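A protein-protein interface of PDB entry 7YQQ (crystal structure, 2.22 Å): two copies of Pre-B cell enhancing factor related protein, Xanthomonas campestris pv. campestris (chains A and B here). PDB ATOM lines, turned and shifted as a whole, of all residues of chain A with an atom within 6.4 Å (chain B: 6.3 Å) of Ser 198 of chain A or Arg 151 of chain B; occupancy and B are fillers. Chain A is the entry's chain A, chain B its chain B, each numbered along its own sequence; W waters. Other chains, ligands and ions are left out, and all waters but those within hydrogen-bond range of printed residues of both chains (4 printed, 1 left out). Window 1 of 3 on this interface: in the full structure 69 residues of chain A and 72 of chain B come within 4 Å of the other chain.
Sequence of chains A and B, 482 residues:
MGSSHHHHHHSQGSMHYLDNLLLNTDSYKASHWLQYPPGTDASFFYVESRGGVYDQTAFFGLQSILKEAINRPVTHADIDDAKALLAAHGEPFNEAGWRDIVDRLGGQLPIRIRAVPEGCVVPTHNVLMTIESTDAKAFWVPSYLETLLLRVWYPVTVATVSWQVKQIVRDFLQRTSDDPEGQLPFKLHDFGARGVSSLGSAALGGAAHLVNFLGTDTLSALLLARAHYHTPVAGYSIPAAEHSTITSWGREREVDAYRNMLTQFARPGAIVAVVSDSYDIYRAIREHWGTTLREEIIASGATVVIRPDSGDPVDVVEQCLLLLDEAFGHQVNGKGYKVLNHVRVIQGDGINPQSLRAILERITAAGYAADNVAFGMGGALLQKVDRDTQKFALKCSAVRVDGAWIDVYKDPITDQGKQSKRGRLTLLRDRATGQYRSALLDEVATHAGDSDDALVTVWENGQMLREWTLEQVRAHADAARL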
ATOM      1  N   GLY A 192     -29.311  16.680  11.977  1.00  0.00           N
ATOM      2  CA  GLY A 192     -28.206  15.918  12.526  1.00  0.00           C
ATOM      3  C   GLY A 192     -27.647  14.745  11.740  1.00  0.00           C
ATOM      4  O   GLY A 192     -26.785  14.039  12.271  1.00  0.00           O
ATOM      5  N   ALA A 193     -28.083  14.505  10.503  1.00  0.00           N
ATOM      6  CA  ALA A 193     -27.640  13.306   9.795  1.00  0.00           C
ATOM      7  C   ALA A 193     -26.116  13.288   9.574  1.00  0.00           C
ATOM      8  O   ALA A 193     -25.491  12.222   9.627  1.00  0.00           O
ATOM      9  CB  ALA A 193     -28.388  13.197   8.471  1.00  0.00           C
ATOM     10  N   ARG A 194     -25.501  14.449   9.349  1.00  0.00           N
ATOM     11  CA  ARG A 194     -24.065  14.509   9.138  1.00  0.00           C
ATOM     12  C   ARG A 194     -23.283  14.508  10.449  1.00  0.00           C
ATOM     13  O   ARG A 194     -22.086  14.218  10.445  1.00  0.00           O
ATOM     14  CB  ARG A 194     -23.716  15.773   8.336  1.00  0.00           C
ATOM     15  CG  ARG A 194     -23.538  17.047   9.211  1.00  0.00           C
ATOM     16  CD  ARG A 194     -23.549  18.347   8.392  1.00  0.00           C
ATOM     17  NE  ARG A 194     -24.555  18.319   7.331  1.00  0.00           N
ATOM     18  CZ  ARG A 194     -24.640  19.211   6.348  1.00  0.00           C
ATOM     19  NH1 ARG A 194     -23.790  20.223   6.279  1.00  0.00           N
ATOM     20  NH2 ARG A 194     -25.576  19.090   5.423  1.00  0.00           N
ATOM     21  N   GLY A 195     -23.922  14.852  11.557  1.00  0.00           N
ATOM     22  CA  GLY A 195     -23.248  15.051  12.813  1.00  0.00           C
ATOM     23  C   GLY A 195     -23.396  13.905  13.772  1.00  0.00           C
ATOM     24  O   GLY A 195     -22.946  14.021  14.917  1.00  0.00           O
ATOM     25  N   VAL A 196     -24.022  12.808  13.342  1.00  0.00           N
ATOM     26  CA  VAL A 196     -24.277  11.648  14.188  1.00  0.00           C
ATOM     27  C   VAL A 196     -23.317  10.537  13.751  1.00  0.00           C
ATOM     28  O   VAL A 196     -22.714  10.586  12.675  1.00  0.00           O
ATOM     29  CB  VAL A 196     -25.788  11.222  14.126  1.00  0.00           C
ATOM     30  CG1 VAL A 196     -26.154  10.627  12.752  1.00  0.00           C
ATOM     31  CG2 VAL A 196     -26.161  10.276  15.251  1.00  0.00           C
ATOM     32  N   SER A 197     -23.139   9.524  14.607  1.00  0.00           N
ATOM     33  CA  SER A 197     -21.979   8.643  14.449  1.00  0.00           C
ATOM     34  C   SER A 197     -22.174   7.509  13.442  1.00  0.00           C
ATOM     35  O   SER A 197     -21.173   6.888  13.056  1.00  0.00           O
ATOM     36  CB  SER A 197     -21.563   8.049  15.805  1.00  0.00           C
ATOM     37  OG  SER A 197     -22.691   7.491  16.462  1.00  0.00           O
ATOM     38  N   SER A 198     -23.402   7.213  13.003  1.00  0.00           N
ATOM     39  CA  SER A 198     -23.577   6.223  11.942  1.00  0.00           C
ATOM     40  C   SER A 198     -24.958   6.398  11.316  1.00  0.00           C
ATOM     41  O   SER A 198     -25.809   7.153  11.806  1.00  0.00           O
ATOM     42  CB  SER A 198     -23.426   4.772  12.455  1.00  0.00           C
ATOM     43  OG  SER A 198     -24.492   4.481  13.381  1.00  0.00           O
ATOM     44  N   LEU A 199     -25.181   5.624  10.252  1.00  0.00           N
ATOM     45  CA  LEU A 199     -26.446   5.632   9.533  1.00  0.00           C
ATOM     46  C   LEU A 199     -27.575   5.082  10.399  1.00  0.00           C
ATOM     47  O   LEU A 199     -28.686   5.632  10.404  1.00  0.00           O
ATOM     48  CB  LEU A 199     -26.304   4.806   8.256  1.00  0.00           C
ATOM     49  CG  LEU A 199     -27.573   4.469   7.477  1.00  0.00           C
ATOM     50  CD1 LEU A 199     -28.267   5.752   7.045  1.00  0.00           C
ATOM     51  CD2 LEU A 199     -27.199   3.638   6.259  1.00  0.00           C
ATOM     52  N   GLY A 200     -27.303   4.012  11.151  1.00  0.00           N
ATOM     53  CA  GLY A 200     -28.337   3.434  11.996  1.00  0.00           C
ATOM     54  C   GLY A 200     -28.725   4.359  13.133  1.00  0.00           C
ATOM     55  O   GLY A 200     -29.901   4.429  13.512  1.00  0.00           O
ATOM     56  N   SER A 201     -27.752   5.099  13.690  1.00  0.00           N
ATOM     57  CA  SER A 201     -28.115   6.058  14.738  1.00  0.00           C
ATOM     58  C   SER A 201     -28.875   7.244  14.151  1.00  0.00           C
ATOM     59  O   SER A 201     -29.801   7.768  14.787  1.00  0.00           O
ATOM     60  CB  SER A 201     -26.881   6.549  15.505  1.00  0.00           C
ATOM     61  OG  SER A 201     -26.192   5.484  16.147  1.00  0.00           O
ATOM     62  N   ALA A 202     -28.504   7.682  12.935  1.00  0.00           N
ATOM     63  CA  ALA A 202     -29.266   8.741  12.267  1.00  0.00           C
ATOM     64  C   ALA A 202     -30.729   8.338  12.105  1.00  0.00           C
ATOM     65  O   ALA A 202     -31.633   9.119  12.389  1.00  0.00           O
ATOM     66  CB  ALA A 202     -28.654   9.075  10.902  1.00  0.00           C
ATOM     67  N   ALA A 203     -30.975   7.110  11.649  1.00  0.00           N
ATOM     68  CA  ALA A 203     -32.343   6.655  11.462  1.00  0.00           C
ATOM     69  C   ALA A 203     -33.086   6.583  12.798  1.00  0.00           C
ATOM     70  O   ALA A 203     -34.230   7.054  12.912  1.00  0.00           O
ATOM     71  CB  ALA A 203     -32.342   5.290  10.750  1.00  0.00           C
ATOM     72  N   SER A 220     -33.095   9.233   6.728  1.00  0.00           N
ATOM     73  CA  SER A 220     -33.007   7.910   7.339  1.00  0.00           C
ATOM     74  C   SER A 220     -34.102   7.679   8.376  1.00  0.00           C
ATOM     75  O   SER A 220     -34.492   6.527   8.604  1.00  0.00           O
ATOM     76  CB  SER A 220     -31.635   7.718   7.991  1.00  0.00           C
ATOM     77  OG  SER A 220     -30.605   8.019   7.079  1.00  0.00           O
ATOM     78  N   GLN A 383     -26.275  13.448  18.597  1.00  0.00           N
ATOM     79  CA  GLN A 383     -24.952  12.969  18.992  1.00  0.00           C
ATOM     80  C   GLN A 383     -24.562  13.347  20.413  1.00  0.00           C
ATOM     81  O   GLN A 383     -23.947  12.540  21.112  1.00  0.00           O
ATOM     82  CB  GLN A 383     -23.881  13.505  18.004  1.00  0.00           C
ATOM     83  CG  GLN A 383     -22.491  12.925  18.186  1.00  0.00           C
ATOM     84  CD  GLN A 383     -22.506  11.392  18.146  1.00  0.00           C
ATOM     85  OE1 GLN A 383     -23.292  10.803  17.380  1.00  0.00           O
ATOM     86  NE2 GLN A 383     -21.651  10.739  18.965  1.00  0.00           N
ATOM     87  N   ASN B  24     -29.768   8.284   1.530  1.00  0.00           N
ATOM     88  CA  ASN B  24     -28.756   8.402   2.580  1.00  0.00           C
ATOM     89  C   ASN B  24     -28.086   9.775   2.486  1.00  0.00           C
ATOM     90  O   ASN B  24     -26.903   9.923   2.131  1.00  0.00           O
ATOM     91  CB  ASN B  24     -27.732   7.268   2.465  1.00  0.00           C
ATOM     92  CG  ASN B  24     -26.751   7.217   3.669  1.00  0.00           C
ATOM     93  OD1 ASN B  24     -26.859   8.017   4.614  1.00  0.00           O
ATOM     94  ND2 ASN B  24     -25.818   6.262   3.641  1.00  0.00           N
ATOM     95  N   THR B  25     -28.856  10.789   2.865  1.00  0.00           N
ATOM     96  CA  THR B  25     -28.435  12.175   2.711  1.00  0.00           C
ATOM     97  C   THR B  25     -29.436  13.077   3.434  1.00  0.00           C
ATOM     98  O   THR B  25     -30.473  12.623   3.934  1.00  0.00           O
ATOM     99  CB  THR B  25     -28.336  12.539   1.224  1.00  0.00           C
ATOM    100  OG1 THR B  25     -27.713  13.811   1.077  1.00  0.00           O
ATOM    101  CG2 THR B  25     -29.723  12.579   0.567  1.00  0.00           C
ATOM    102  N   ILE B  65     -16.924   3.012   5.581  1.00  0.00           N
ATOM    103  CA  ILE B  65     -18.058   3.817   5.148  1.00  0.00           C
ATOM    104  C   ILE B  65     -18.364   3.556   3.683  1.00  0.00           C
ATOM    105  O   ILE B  65     -19.519   3.353   3.314  1.00  0.00           O
ATOM    106  CB  ILE B  65     -17.785   5.305   5.411  1.00  0.00           C
ATOM    107  CG1 ILE B  65     -17.899   5.590   6.904  1.00  0.00           C
ATOM    108  CG2 ILE B  65     -18.759   6.198   4.598  1.00  0.00           C
ATOM    109  CD1 ILE B  65     -17.548   7.061   7.276  1.00  0.00           C
ATOM    110  N   ALA B  69     -21.889   2.001   2.639  1.00  0.00           N
ATOM    111  CA  ALA B  69     -22.836   2.980   2.115  1.00  0.00           C
ATOM    112  C   ALA B  69     -22.932   2.932   0.597  1.00  0.00           C
ATOM    113  O   ALA B  69     -23.972   3.301   0.037  1.00  0.00           O
ATOM    114  CB  ALA B  69     -22.429   4.393   2.563  1.00  0.00           C
ATOM    115  N   GLU B 146     -22.161  14.395   0.775  1.00  0.00           N
ATOM    116  CA  GLU B 146     -21.546  15.038   1.938  1.00  0.00           C
ATOM    117  C   GLU B 146     -22.025  14.416   3.245  1.00  0.00           C
ATOM    118  O   GLU B 146     -21.216  14.142   4.140  1.00  0.00           O
ATOM    119  CB  GLU B 146     -21.826  16.546   1.954  1.00  0.00           C
ATOM    120  CG  GLU B 146     -21.487  17.154   3.345  1.00  0.00           C
ATOM    121  CD  GLU B 146     -21.617  18.669   3.430  1.00  0.00           C
ATOM    122  OE1 GLU B 146     -20.867  19.306   4.212  1.00  0.00           O
ATOM    123  OE2 GLU B 146     -22.477  19.226   2.721  1.00  0.00           O
ATOM    124  N   THR B 147     -23.333  14.173   3.373  1.00  0.00           N
ATOM    125  CA  THR B 147     -23.876  13.721   4.648  1.00  0.00           C
ATOM    126  C   THR B 147     -23.237  12.405   5.085  1.00  0.00           C
ATOM    127  O   THR B 147     -22.765  12.276   6.220  1.00  0.00           O
ATOM    128  CB  THR B 147     -25.398  13.570   4.553  1.00  0.00           C
ATOM    129  OG1 THR B 147     -25.968  14.690   3.850  1.00  0.00           O
ATOM    130  CG2 THR B 147     -25.997  13.509   5.945  1.00  0.00           C
ATOM    131  N   LEU B 148     -23.209  11.410   4.197  1.00  0.00           N
ATOM    132  CA  LEU B 148     -22.652  10.142   4.623  1.00  0.00           C
ATOM    133  C   LEU B 148     -21.134  10.180   4.672  1.00  0.00           C
ATOM    134  O   LEU B 148     -20.539   9.412   5.431  1.00  0.00           O
ATOM    135  CB  LEU B 148     -23.114   9.001   3.716  1.00  0.00           C
ATOM    136  CG  LEU B 148     -22.546   8.907   2.298  1.00  0.00           C
ATOM    137  CD1 LEU B 148     -21.211   8.138   2.268  1.00  0.00           C
ATOM    138  CD2 LEU B 148     -23.563   8.267   1.338  1.00  0.00           C
ATOM    139  N   LEU B 149     -20.481  11.032   3.881  1.00  0.00           N
ATOM    140  CA  LEU B 149     -19.020  11.039   3.978  1.00  0.00           C
ATOM    141  C   LEU B 149     -18.551  11.799   5.208  1.00  0.00           C
ATOM    142  O   LEU B 149     -17.580  11.392   5.850  1.00  0.00           O
ATOM    143  CB  LEU B 149     -18.382  11.636   2.724  1.00  0.00           C
ATOM    144  CG  LEU B 149     -18.515  10.781   1.454  1.00  0.00           C
ATOM    145  CD1 LEU B 149     -18.091  11.575   0.233  1.00  0.00           C
ATOM    146  CD2 LEU B 149     -17.705   9.491   1.589  1.00  0.00           C
ATOM    147  N   LEU B 150     -19.203  12.912   5.545  1.00  0.00           N
ATOM    148  CA  LEU B 150     -18.740  13.688   6.690  1.00  0.00           C
ATOM    149  C   LEU B 150     -18.863  12.912   8.001  1.00  0.00           C
ATOM    150  O   LEU B 150     -18.177  13.241   8.977  1.00  0.00           O
ATOM    151  CB  LEU B 150     -19.508  15.010   6.751  1.00  0.00           C
ATOM    152  CG  LEU B 150     -19.045  16.116   7.707  1.00  0.00           C
ATOM    153  CD1 LEU B 150     -17.543  16.272   7.673  1.00  0.00           C
ATOM    154  CD2 LEU B 150     -19.736  17.445   7.349  1.00  0.00           C
ATOM    155  N   ARG B 151     -19.711  11.875   8.042  1.00  0.00           N
ATOM    156  CA  ARG B 151     -19.784  10.996   9.207  1.00  0.00           C
ATOM    157  C   ARG B 151     -18.457  10.274   9.464  1.00  0.00           C
ATOM    158  O   ARG B 151     -18.302   9.589  10.492  1.00  0.00           O
ATOM    159  CB  ARG B 151     -20.946  10.014   9.017  1.00  0.00           C
ATOM    160  CG  ARG B 151     -22.342  10.650   9.313  1.00  0.00           C
ATOM    161  CD  ARG B 151     -23.423   9.582   9.661  1.00  0.00           C
ATOM    162  NE  ARG B 151     -23.802   8.800   8.481  1.00  0.00           N
ATOM    163  CZ  ARG B 151     -24.927   8.974   7.774  1.00  0.00           C
ATOM    164  NH1 ARG B 151     -25.829   9.903   8.128  1.00  0.00           N
ATOM    165  NH2 ARG B 151     -25.161   8.207   6.707  1.00  0.00           N
ATOM    166  N   VAL B 152     -17.485  10.428   8.566  1.00  0.00           N
ATOM    167  CA  VAL B 152     -16.169   9.898   8.842  1.00  0.00           C
ATOM    168  C   VAL B 152     -15.545  10.573  10.056  1.00  0.00           C
ATOM    169  O   VAL B 152     -14.583  10.040  10.628  1.00  0.00           O
ATOM    170  CB  VAL B 152     -15.293  10.042   7.597  1.00  0.00           C
ATOM    171  CG1 VAL B 152     -14.824  11.507   7.453  1.00  0.00           C
ATOM    172  CG2 VAL B 152     -14.140   9.073   7.672  1.00  0.00           C
ATOM    173  N   TRP B 153     -16.092  11.721  10.486  1.00  0.00           N
ATOM    174  CA  TRP B 153     -15.613  12.370  11.703  1.00  0.00           C
ATOM    175  C   TRP B 153     -15.606  11.402  12.876  1.00  0.00           C
ATOM    176  O   TRP B 153     -14.782  11.537  13.790  1.00  0.00           O
ATOM    177  CB  TRP B 153     -16.472  13.613  12.051  1.00  0.00           C
ATOM    178  CG  TRP B 153     -17.828  13.266  12.589  1.00  0.00           C
ATOM    179  CD1 TRP B 153     -19.008  13.255  11.891  1.00  0.00           C
ATOM    180  CD2 TRP B 153     -18.143  12.817  13.915  1.00  0.00           C
ATOM    181  NE1 TRP B 153     -20.042  12.841  12.701  1.00  0.00           N
ATOM    182  CE2 TRP B 153     -19.540  12.562  13.951  1.00  0.00           C
ATOM    183  CE3 TRP B 153     -17.398  12.645  15.083  1.00  0.00           C
ATOM    184  CZ2 TRP B 153     -20.195  12.113  15.112  1.00  0.00           C
ATOM    185  CZ3 TRP B 153     -18.057  12.191  16.240  1.00  0.00           C
ATOM    186  CH2 TRP B 153     -19.440  11.920  16.234  1.00  0.00           C
ATOM    187  N   TYR B 154     -16.519  10.438  12.882  1.00  0.00           N
ATOM    188  CA  TYR B 154     -16.703   9.598  14.058  1.00  0.00           C
ATOM    189  C   TYR B 154     -15.591   8.563  14.189  1.00  0.00           C
ATOM    190  O   TYR B 154     -14.931   8.534  15.238  1.00  0.00           O
ATOM    191  CB  TYR B 154     -18.075   8.925  14.050  1.00  0.00           C
ATOM    192  CG  TYR B 154     -18.220   7.922  15.164  1.00  0.00           C
ATOM    193  CD1 TYR B 154     -18.138   8.323  16.497  1.00  0.00           C
ATOM    194  CD2 TYR B 154     -18.432   6.569  14.889  1.00  0.00           C
ATOM    195  CE1 TYR B 154     -18.273   7.409  17.528  1.00  0.00           C
ATOM    196  CE2 TYR B 154     -18.563   5.645  15.916  1.00  0.00           C
ATOM    197  CZ  TYR B 154     -18.485   6.083  17.230  1.00  0.00           C
ATOM    198  OH  TYR B 154     -18.624   5.183  18.253  1.00  0.00           O
ATOM    199  N   PRO B 155     -15.333   7.704  13.186  1.00  0.00           N
ATOM    200  CA  PRO B 155     -14.154   6.822  13.329  1.00  0.00           C
ATOM    201  C   PRO B 155     -12.858   7.607  13.469  1.00  0.00           C
ATOM    202  O   PRO B 155     -11.969   7.192  14.227  1.00  0.00           O
ATOM    203  CB  PRO B 155     -14.181   5.952  12.057  1.00  0.00           C
ATOM    204  CG  PRO B 155     -15.076   6.679  11.083  1.00  0.00           C
ATOM    205  CD  PRO B 155     -16.061   7.456  11.915  1.00  0.00           C
ATOM    206  N   VAL B 156     -12.725   8.747  12.794  1.00  0.00           N
ATOM    207  CA  VAL B 156     -11.493   9.529  12.942  1.00  0.00           C
ATOM    208  C   VAL B 156     -11.316   9.966  14.388  1.00  0.00           C
ATOM    209  O   VAL B 156     -10.211   9.920  14.945  1.00  0.00           O
ATOM    210  CB  VAL B 156     -11.499  10.761  12.018  1.00  0.00           C
ATOM    211  CG1 VAL B 156     -10.381  11.699  12.426  1.00  0.00           C
ATOM    212  CG2 VAL B 156     -11.391  10.373  10.535  1.00  0.00           C
ATOM    213  N   SER B 197     -24.624   4.740  20.643  1.00  0.00           N
ATOM    214  CA  SER B 197     -25.993   4.974  20.199  1.00  0.00           C
ATOM    215  C   SER B 197     -26.570   3.843  19.353  1.00  0.00           C
ATOM    216  O   SER B 197     -27.795   3.726  19.287  1.00  0.00           O
ATOM    217  CB  SER B 197     -26.095   6.292  19.424  1.00  0.00           C
ATOM    218  OG  SER B 197     -25.084   6.386  18.444  1.00  0.00           O
ATOM    219  N   SER B 198     -25.756   3.019  18.697  1.00  0.00           N
ATOM    220  CA  SER B 198     -26.342   1.977  17.864  1.00  0.00           C
ATOM    221  C   SER B 198     -25.323   0.883  17.620  1.00  0.00           C
ATOM    222  O   SER B 198     -24.137   1.024  17.917  1.00  0.00           O
ATOM    223  CB  SER B 198     -26.837   2.522  16.518  1.00  0.00           C
ATOM    224  OG  SER B 198     -25.735   2.926  15.707  1.00  0.00           O
ATOM    225  N   LEU B 199     -25.815  -0.202  17.027  1.00  0.00           N
ATOM    226  CA  LEU B 199     -24.958  -1.338  16.722  1.00  0.00           C
ATOM    227  C   LEU B 199     -23.890  -0.950  15.709  1.00  0.00           C
ATOM    228  O   LEU B 199     -22.713  -1.292  15.873  1.00  0.00           O
ATOM    229  CB  LEU B 199     -25.820  -2.495  16.212  1.00  0.00           C
ATOM    230  CG  LEU B 199     -25.121  -3.697  15.595  1.00  0.00           C
ATOM    231  CD1 LEU B 199     -24.122  -4.279  16.587  1.00  0.00           C
ATOM    232  CD2 LEU B 199     -26.193  -4.714  15.220  1.00  0.00           C
ATOM    233  N   GLY B 200     -24.279  -0.206  14.671  1.00  0.00           N
ATOM    234  CA  GLY B 200     -23.323   0.186  13.651  1.00  0.00           C
ATOM    235  C   GLY B 200     -22.265   1.141  14.174  1.00  0.00           C
ATOM    236  O   GLY B 200     -21.085   1.031  13.820  1.00  0.00           O
ATOM    237  N   SER B 201     -22.666   2.077  15.036  1.00  0.00           N
ATOM    238  CA  SER B 201     -21.689   2.923  15.712  1.00  0.00           C
ATOM    239  C   SER B 201     -20.757   2.092  16.590  1.00  0.00           C
ATOM    240  O   SER B 201     -19.542   2.330  16.625  1.00  0.00           O
ATOM    241  CB  SER B 201     -22.412   3.972  16.546  1.00  0.00           C
ATOM    242  OG  SER B 201     -23.037   4.929  15.713  1.00  0.00           O
ATOM    243  N   ALA B 202     -21.313   1.122  17.323  1.00  0.00           N
ATOM    244  CA  ALA B 202     -20.479   0.254  18.145  1.00  0.00           C
ATOM    245  C   ALA B 202     -19.432  -0.451  17.301  1.00  0.00           C
ATOM    246  O   ALA B 202     -18.263  -0.531  17.690  1.00  0.00           O
ATOM    247  CB  ALA B 202     -21.334  -0.783  18.887  1.00  0.00           C
ATOM    248  N   LEU B 204     -18.176   0.344  14.247  1.00  0.00           N
ATOM    249  CA  LEU B 204     -17.221   1.235  13.610  1.00  0.00           C
ATOM    250  C   LEU B 204     -16.337   1.949  14.633  1.00  0.00           C
ATOM    251  O   LEU B 204     -15.118   2.020  14.451  1.00  0.00           O
ATOM    252  CB  LEU B 204     -17.962   2.240  12.728  1.00  0.00           C
ATOM    253  CG  LEU B 204     -17.133   3.267  11.919  1.00  0.00           C
ATOM    254  CD1 LEU B 204     -15.929   2.606  11.084  1.00  0.00           C
ATOM    255  CD2 LEU B 204     -18.083   4.158  11.045  1.00  0.00           C
HETATM  256  O   HOH W   1     -28.265   9.482   6.569  1.00  0.00           O
HETATM  257  O   HOH W   2     -19.319   7.219  10.966  1.00  0.00           O
HETATM  258  O   HOH W   3     -30.698  11.052   6.400  1.00  0.00           O
HETATM  259  O   HOH W   4     -25.022   9.150  18.508  1.00  0.00           O
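The side-chain hydroxyl (OG) of Ser 198 of chain A sits at hydrogen-bond distance from the side-chain hydroxyl (OG) of Ser 198 of chain B.
The side-chain hydroxyl of Ser 201 of chain B sits at hydrogen-bond distance from the side-chain hydroxyl of Ser 201 of chain A, 3.2 Å away.
OE1 of Glu 146 of chain B is in salt-bridge range of NH1 of Arg 194 of chain A (3.7 Å).
The side-chain hydroxyl of Ser 201 of chain B lies within hydrogen-bond range of the side-chain hydroxyl of Ser 198 of chain A (2.8 Å).
O of Arg 194 of chain A is in hydrogen-bond range of NE1 of Trp 153 of chain B, at 3.3 Å.
The side-chain hydroxyl of Ser 197 of chain A is in hydrogen-bond range of the side-chain hydroxyl of Ser 197 of chain B (3.3 Å).
The side-chain hydroxyl of Ser 197 of chain B is in hydrogen-bond range of the side-chain hydroxyl of Ser 201 of chain A (2.7 Å).
The side-chain hydroxyl (OG) of Ser 201 of chain B lies within hydrogen-bond range of the side-chain hydroxyl (OG) of Ser 197 of chain A, at 2.7 Å.
The guanidinium group (NH1) of Arg 151 of chain B sits at hydrogen-bond distance from the backbone carbonyl oxygen (O) of Ala 193 of chain A (2.8 Å).
OG of Ser 198 of chain B lies within hydrogen-bond range of OG of Ser 201 of chain A.
The backbone carbonyl oxygen of Val 196 of chain A lies within hydrogen-bond range of the indole nitrogen of Trp 153 of chain B.
OD1 of Asn 24 of chain B sits at hydrogen-bond distance from NH2 of Arg 151 of chain B (2.7 Å).
N of Ser 201 of chain B lies within hydrogen-bond range of OG of Ser 198 of chain B, at 3.3 Å.
OG of Ser 198 of chain A is in hydrogen-bond range of N of Ser 201 of chain A, 3.3 Å away.
The side-chain hydroxyl (OG1) of Thr 147 of chain B sits at hydrogen-bond distance from the side-chain hydroxyl (OG1) of Thr 25 of chain B, 3.4 Å away.
N of Ser 197 of chain A lies within hydrogen-bond range of OE1 of Gln 383 of chain A, at 3.1 Å.
The backbone carbonyl oxygen (O) of Ser 201 of chain B lies within hydrogen-bond range of the side-chain hydroxyl (OH) of Tyr 154 of chain B.
Thr 147 of chain B touches Ala 193 of chain A.
CG2 of Thr 147 of chain B touches N of Arg 194 of chain A (3.6 Å).
Arg 194 of chain A touches Arg 151 of chain B (O to CG, 3.8 Å).
Val 196 of chain A touches Arg 151 of chain B (O to CD, 3.3 Å).
Ser 197 of chain A touches Trp 153 of chain B.
Ser 197 of chain A touches Tyr 154 of chain B (O to CD2, 3.3 Å).
Arg 151 of chain B touches Ser 198 of chain A.
Leu 199 of chain A touches Asn 24 of chain B.
Leu 199 of chain A touches Arg 151 of chain B.
Trp 153 of chain B touches Gln 383 of chain A.
Printed residues of chain B within 4 Å of Arg 194 of chain A: Glu 146, Thr 147, Arg 151 and Trp 153.
Ser 198 of chain A touches just these residues of chain B: Arg 151 (3.9 Å), Ser 198 (3.1 Å) and Ser 201 (2.8 Å).
Gly 200 of chain A touches none of the printed residues of chain B.
Of chain A, only Ala 193, Arg 194, Val 196, Ser 198 and Leu 199 come within 4 Å of Arg 151 of chain B.
Of the printed residues of chain A, Tyr 154 of chain B touches Ser 197.
Of the printed residues of chain A, Ser 198 of chain B touches Ser 198 (3.1 Å) and Ser 201 (2.6 Å).
Printed residues of chain A within 4 Å of Ser 201 of chain B: Ser 197, Ser 198 and Ser 201.
The nearest residue of chain B that does not touch Ser 198 of chain A is Gly 200 of chain B (4.1 Å).
The nearest residue of chain A that does not touch Arg 151 of chain B is Ala 202 of chain A (4.04 Å).
The nearest printed residue of chain B that does not touch Gly 195 of chain A is Arg 151 of chain B (5.0 Å).
Hydrophobic or aromatic side chains of chain B that line the printed part of chain A: Trp 153 and Tyr 154.
Printed residues of chain A that touch a printed residue of chain B: Ala 193, Arg 194, Gly 195, Val 196, Ser 197, Ser 198, Leu 199, Ser 201 and Gln 383.
Hydrophobic or aromatic side chains of chain A that line the printed part of chain B: Ala 193 and Leu 199.
Among the printed residues, Asp or Glu carboxylates within 4 Å of a Lys or Arg side-chain nitrogen of the other chain: Arg 194 of chain A with Glu 146 of chain B (3.7 Å).
Ser 197 of chain B touches its own counterpart, Ser 197 of chain A.
Ser 197 of chain A touches Ser 201 of chain B, and with the chains exchanged Ser 201 of chain A touches Ser 197 of chain B.
Ser 198 of chain A touches its own counterpart, Ser 198 of chain B.
Ser 198 of chain A touches Ser 201 of chain B, and with the chains exchanged Ser 201 of chain A touches Ser 198 of chain B.
6 positions are printed for both chains.
Water W2 lies within hydrogen-bond range of the backbone carbonyl oxygen (O) of Arg 151 of chain B and the backbone carbonyl oxygen (O) of Ser 197 of chain A.
Water W4 lies within hydrogen-bond range of OE1 of Gln 383 of chain A (2.6 Å) and OG of Ser 197 of chain B (2.8 Å).
Water W1 lies within hydrogen-bond range of the side-chain hydroxyl of Ser 220 of chain A, the side-chain amide oxygen of Asn 24 of chain B and the guanidinium group of Arg 151 of chain B.
Water W3 lies within hydrogen-bond range of O of Thr 25 of chain B (2.9 Å) and N of Ser 220 of chain A (3.0 Å).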
